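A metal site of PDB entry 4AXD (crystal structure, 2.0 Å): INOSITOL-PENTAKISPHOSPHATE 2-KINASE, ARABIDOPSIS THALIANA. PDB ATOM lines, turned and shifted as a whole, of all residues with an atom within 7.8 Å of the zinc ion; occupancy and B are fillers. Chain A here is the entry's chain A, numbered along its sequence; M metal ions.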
ATOM      1  N   GLU A 321      10.316 -10.488  25.288  1.00  0.00           N
ATOM      2  CA  GLU A 321      10.219 -11.205  23.994  1.00  0.00           C
ATOM      3  C   GLU A 321      10.399 -12.709  24.143  1.00  0.00           C
ATOM      4  O   GLU A 321       9.865 -13.492  23.351  1.00  0.00           O
ATOM      5  CB  GLU A 321      11.264 -10.691  23.013  1.00  0.00           C
ATOM      6  CG  GLU A 321      10.801  -9.549  22.132  1.00  0.00           C
ATOM      7  CD  GLU A 321      11.740  -9.338  20.973  1.00  0.00           C
ATOM      8  OE1 GLU A 321      11.763 -10.176  20.051  1.00  0.00           O
ATOM      9  OE2 GLU A 321      12.481  -8.355  20.975  1.00  0.00           O
ATOM     10  N   GLY A 322      11.179 -13.112  25.137  1.00  0.00           N
ATOM     11  CA  GLY A 322      11.362 -14.518  25.474  1.00  0.00           C
ATOM     12  C   GLY A 322      10.281 -14.984  26.430  1.00  0.00           C
ATOM     13  O   GLY A 322       9.592 -15.991  26.173  1.00  0.00           O
ATOM     14  N   ILE A 324       7.311 -14.066  27.237  1.00  0.00           N
ATOM     15  CA  ILE A 324       5.919 -14.108  26.808  1.00  0.00           C
ATOM     16  C   ILE A 324       5.520 -15.528  26.363  1.00  0.00           C
ATOM     17  O   ILE A 324       4.380 -15.954  26.559  1.00  0.00           O
ATOM     18  CB  ILE A 324       5.625 -13.016  25.736  1.00  0.00           C
ATOM     19  CG1 ILE A 324       4.112 -12.804  25.523  1.00  0.00           C
ATOM     20  CG2 ILE A 324       6.334 -13.313  24.419  1.00  0.00           C
ATOM     21  CD1 ILE A 324       3.336 -12.320  26.745  1.00  0.00           C
ATOM     22  N   HIS A 325       6.471 -16.276  25.810  1.00  0.00           N
ATOM     23  CA  HIS A 325       6.234 -17.665  25.388  1.00  0.00           C
ATOM     24  C   HIS A 325       6.016 -18.558  26.572  1.00  0.00           C
ATOM     25  O   HIS A 325       5.179 -19.454  26.537  1.00  0.00           O
ATOM     26  CB  HIS A 325       7.397 -18.174  24.555  1.00  0.00           C
ATOM     27  CG  HIS A 325       7.617 -17.393  23.280  1.00  0.00           C
ATOM     28  ND1 HIS A 325       7.100 -17.767  22.095  1.00  0.00           N
ATOM     29  CD2 HIS A 325       8.334 -16.217  23.036  1.00  0.00           C
ATOM     30  CE1 HIS A 325       7.462 -16.879  21.148  1.00  0.00           C
ATOM     31  NE2 HIS A 325       8.205 -15.932  21.728  1.00  0.00           N
ATOM     32  N   CYS A 326       6.744 -18.302  27.656  1.00  0.00           N
ATOM     33  CA  CYS A 326       6.561 -19.056  28.888  1.00  0.00           C
ATOM     34  C   CYS A 326       5.198 -18.728  29.496  1.00  0.00           C
ATOM     35  O   CYS A 326       4.544 -19.609  30.072  1.00  0.00           O
ATOM     36  CB  CYS A 326       7.694 -18.761  29.877  1.00  0.00           C
ATOM     37  SG  CYS A 326       9.346 -19.228  29.313  1.00  0.00           S
ATOM     38  N   TYR A 328       2.347 -18.027  27.907  1.00  0.00           N
ATOM     39  CA  TYR A 328       1.318 -18.813  27.229  1.00  0.00           C
ATOM     40  C   TYR A 328       1.268 -20.272  27.657  1.00  0.00           C
ATOM     41  O   TYR A 328       0.178 -20.832  27.820  1.00  0.00           O
ATOM     42  CB  TYR A 328       1.378 -18.622  25.713  1.00  0.00           C
ATOM     43  CG  TYR A 328       0.803 -17.281  25.365  1.00  0.00           C
ATOM     44  CD1 TYR A 328      -0.551 -17.040  25.526  1.00  0.00           C
ATOM     45  CD2 TYR A 328       1.627 -16.225  24.942  1.00  0.00           C
ATOM     46  CE1 TYR A 328      -1.097 -15.804  25.246  1.00  0.00           C
ATOM     47  CE2 TYR A 328       1.088 -14.988  24.649  1.00  0.00           C
ATOM     48  CZ  TYR A 328      -0.283 -14.790  24.816  1.00  0.00           C
ATOM     49  OH  TYR A 328      -0.853 -13.585  24.546  1.00  0.00           O
ATOM     50  N   ASP A 329       2.435 -20.867  27.889  1.00  0.00           N
ATOM     51  CA  ASP A 329       2.512 -22.221  28.421  1.00  0.00           C
ATOM     52  C   ASP A 329       1.866 -22.316  29.797  1.00  0.00           C
ATOM     53  O   ASP A 329       1.101 -23.253  30.071  1.00  0.00           O
ATOM     54  CB  ASP A 329       3.974 -22.704  28.485  1.00  0.00           C
ATOM     55  CG  ASP A 329       4.524 -23.068  27.123  1.00  0.00           C
ATOM     56  OD1 ASP A 329       3.744 -23.199  26.166  1.00  0.00           O
ATOM     57  OD2 ASP A 329       5.757 -23.229  26.995  1.00  0.00           O
ATOM     58  N   GLN A 333      -2.444 -21.924  27.037  1.00  0.00           N
ATOM     59  CA  GLN A 333      -2.996 -21.479  25.749  1.00  0.00           C
ATOM     60  C   GLN A 333      -2.010 -21.773  24.645  1.00  0.00           C
ATOM     61  O   GLN A 333      -0.795 -21.797  24.890  1.00  0.00           O
ATOM     62  CB  GLN A 333      -3.263 -19.981  25.762  1.00  0.00           C
ATOM     63  CG  GLN A 333      -3.941 -19.472  27.022  1.00  0.00           C
ATOM     64  CD  GLN A 333      -5.397 -19.844  27.124  1.00  0.00           C
ATOM     65  OE1 GLN A 333      -5.825 -20.858  26.573  1.00  0.00           O
ATOM     66  NE2 GLN A 333      -6.174 -19.020  27.829  1.00  0.00           N
ATOM     67  N   PRO A 334      -2.528 -21.979  23.409  1.00  0.00           N
ATOM     68  CA  PRO A 334      -1.639 -21.948  22.256  1.00  0.00           C
ATOM     69  C   PRO A 334      -1.014 -20.564  22.139  1.00  0.00           C
ATOM     70  O   PRO A 334      -1.680 -19.554  22.348  1.00  0.00           O
ATOM     71  CB  PRO A 334      -2.565 -22.236  21.073  1.00  0.00           C
ATOM     72  CG  PRO A 334      -3.712 -22.976  21.680  1.00  0.00           C
ATOM     73  CD  PRO A 334      -3.896 -22.389  23.044  1.00  0.00           C
ATOM     74  N   CYS A 335       0.268 -20.527  21.828  1.00  0.00           N
ATOM     75  CA  CYS A 335       1.012 -19.282  21.810  1.00  0.00           C
ATOM     76  C   CYS A 335       0.770 -18.510  20.506  1.00  0.00           C
ATOM     77  O   CYS A 335       1.036 -19.033  19.435  1.00  0.00           O
ATOM     78  CB  CYS A 335       2.502 -19.608  21.983  1.00  0.00           C
ATOM     79  SG  CYS A 335       3.535 -18.195  22.404  1.00  0.00           S
ATOM     80  N   PRO A 336       0.257 -17.259  20.604  1.00  0.00           N
ATOM     81  CA  PRO A 336       0.042 -16.453  19.388  1.00  0.00           C
ATOM     82  C   PRO A 336       1.307 -15.790  18.857  1.00  0.00           C
ATOM     83  O   PRO A 336       1.337 -15.353  17.718  1.00  0.00           O
ATOM     84  CB  PRO A 336      -0.971 -15.390  19.839  1.00  0.00           C
ATOM     85  CG  PRO A 336      -0.698 -15.218  21.288  1.00  0.00           C
ATOM     86  CD  PRO A 336      -0.266 -16.572  21.800  1.00  0.00           C
ATOM     87  N   ILE A 337       2.348 -15.737  19.685  1.00  0.00           N
ATOM     88  CA  ILE A 337       3.635 -15.173  19.267  1.00  0.00           C
ATOM     89  C   ILE A 337       4.255 -15.998  18.142  1.00  0.00           C
ATOM     90  O   ILE A 337       4.570 -15.474  17.078  1.00  0.00           O
ATOM     91  CB  ILE A 337       4.604 -14.944  20.447  1.00  0.00           C
ATOM     92  CG1 ILE A 337       3.874 -14.361  21.673  1.00  0.00           C
ATOM     93  CG2 ILE A 337       5.794 -14.095  20.011  1.00  0.00           C
ATOM     94  CD1 ILE A 337       3.156 -13.039  21.433  1.00  0.00           C
ATOM     95  N   CYS A 338       4.358 -17.268  18.474  1.00  0.00           N
ATOM     96  CA  CYS A 338       4.738 -18.347  17.614  1.00  0.00           C
ATOM     97  C   CYS A 338       3.883 -18.413  16.356  1.00  0.00           C
ATOM     98  O   CYS A 338       4.347 -18.841  15.362  1.00  0.00           O
ATOM     99  CB  CYS A 338       4.669 -19.652  18.414  1.00  0.00           C
ATOM    100  SG  CYS A 338       6.144 -20.117  19.303  1.00  0.00           S
ATOM    101  N   ARG A 339       2.646 -18.000  16.369  1.00  0.00           N
ATOM    102  CA  ARG A 339       1.938 -17.934  15.081  1.00  0.00           C
ATOM    103  C   ARG A 339       2.281 -16.763  14.134  1.00  0.00           C
ATOM    104  O   ARG A 339       1.884 -16.807  13.007  1.00  0.00           O
ATOM    105  CB  ARG A 339       0.459 -17.835  15.291  1.00  0.00           C
ATOM    106  CG  ARG A 339      -0.131 -18.875  16.128  1.00  0.00           C
ATOM    107  CD  ARG A 339      -1.625 -18.771  16.122  1.00  0.00           C
ATOM    108  NE  ARG A 339      -2.104 -20.005  16.659  1.00  0.00           N
ATOM    109  CZ  ARG A 339      -2.811 -20.143  17.776  1.00  0.00           C
ATOM    110  NH1 ARG A 339      -3.186 -19.084  18.526  1.00  0.00           N
ATOM    111  NH2 ARG A 339      -3.155 -21.372  18.105  1.00  0.00           N
ATOM    112  N   PRO A 343       8.965 -19.119  14.075  1.00  0.00           N
ATOM    113  CA  PRO A 343       9.514 -19.028  15.436  1.00  0.00           C
ATOM    114  C   PRO A 343      11.032 -19.318  15.496  1.00  0.00           C
ATOM    115  O   PRO A 343      11.515 -20.189  14.785  1.00  0.00           O
ATOM    116  CB  PRO A 343       8.749 -20.113  16.210  1.00  0.00           C
ATOM    117  CG  PRO A 343       7.627 -20.532  15.326  1.00  0.00           C
ATOM    118  CD  PRO A 343       8.084 -20.286  13.927  1.00  0.00           C
ATOM    119  N   GLU A 347      12.945 -19.818  20.887  1.00  0.00           N
ATOM    120  CA  GLU A 347      11.550 -19.806  21.356  1.00  0.00           C
ATOM    121  C   GLU A 347      10.979 -21.212  21.517  1.00  0.00           C
ATOM    122  O   GLU A 347      10.301 -21.514  22.508  1.00  0.00           O
ATOM    123  CB  GLU A 347      10.667 -18.995  20.401  1.00  0.00           C
ATOM    124  CG  GLU A 347      11.134 -17.555  20.234  1.00  0.00           C
ATOM    125  CD  GLU A 347      10.367 -16.785  19.179  1.00  0.00           C
ATOM    126  OE1 GLU A 347       9.701 -17.389  18.307  1.00  0.00           O
ATOM    127  OE2 GLU A 347      10.443 -15.536  19.222  1.00  0.00           O
ATOM    128  N   LEU A 348      11.258 -22.068  20.546  1.00  0.00           N
ATOM    129  CA  LEU A 348      10.817 -23.468  20.585  1.00  0.00           C
ATOM    130  C   LEU A 348      11.393 -24.197  21.788  1.00  0.00           C
ATOM    131  O   LEU A 348      10.684 -24.942  22.459  1.00  0.00           O
ATOM    132  CB  LEU A 348      11.213 -24.191  19.296  1.00  0.00           C
ATOM    133  CG  LEU A 348      10.519 -23.692  18.023  1.00  0.00           C
ATOM    134  CD1 LEU A 348      11.036 -24.456  16.821  1.00  0.00           C
ATOM    135  CD2 LEU A 348       9.000 -23.821  18.139  1.00  0.00           C
ATOM    136  N   LEU A 350      12.103 -22.854  24.558  1.00  0.00           N
ATOM    137  CA  LEU A 350      11.353 -22.368  25.731  1.00  0.00           C
ATOM    138  C   LEU A 350      10.080 -23.175  25.931  1.00  0.00           C
ATOM    139  O   LEU A 350       9.784 -23.603  27.049  1.00  0.00           O
ATOM    140  CB  LEU A 350      11.048 -20.877  25.635  1.00  0.00           C
ATOM    141  CG  LEU A 350      12.222 -19.878  25.661  1.00  0.00           C
ATOM    142  CD1 LEU A 350      11.709 -18.453  25.541  1.00  0.00           C
ATOM    143  CD2 LEU A 350      13.076 -20.056  26.902  1.00  0.00           C
ATOM    144  N   HIS A 351       9.334 -23.399  24.846  1.00  0.00           N
ATOM    145  CA  HIS A 351       8.105 -24.198  24.918  1.00  0.00           C
ATOM    146  C   HIS A 351       8.364 -25.640  25.287  1.00  0.00           C
ATOM    147  O   HIS A 351       7.493 -26.315  25.835  1.00  0.00           O
ATOM    148  CB  HIS A 351       7.315 -24.107  23.620  1.00  0.00           C
ATOM    149  CG  HIS A 351       6.639 -22.768  23.418  1.00  0.00           C
ATOM    150  ND1 HIS A 351       5.654 -22.320  24.231  1.00  0.00           N
ATOM    151  CD2 HIS A 351       6.845 -21.764  22.464  1.00  0.00           C
ATOM    152  CE1 HIS A 351       5.234 -21.108  23.801  1.00  0.00           C
ATOM    153  NE2 HIS A 351       5.968 -20.761  22.729  1.00  0.00           N
HETATM  154 ZN    ZN M   1       5.560 -19.132  21.574  1.00  0.00          ZN
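The zinc ion is bound by a ring nitrogen (NE2) of His 351 (2.0 Å), a ring nitrogen (ND1) of His 325 (2.1 Å), the side-chain sulfur (SG) of Cys 335 (2.4 Å) and the side-chain sulfur (SG) of Cys 338 (2.5 Å). The zinc ion has four donor atoms within binding distance.
Within 4 Å of the zinc ion: His 325, Cys 335, Cys 338 and His 351. The nearest printed residue that does not touch the zinc ion is Ile 337 (4.4 Å).
A ring nitrogen (ND1) of His 351 is in hydrogen-bond range of the side-chain carboxylate (OD1) of Asp 329, at 2.9 Å. A ring nitrogen (NE2) of His 325 lies within hydrogen-bond range of the side-chain carboxylate of Glu 347. The backbone carbonyl oxygen (O) of Glu 321 sits close to a ring nitrogen (NE2) of His 325 (3.4 Å).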
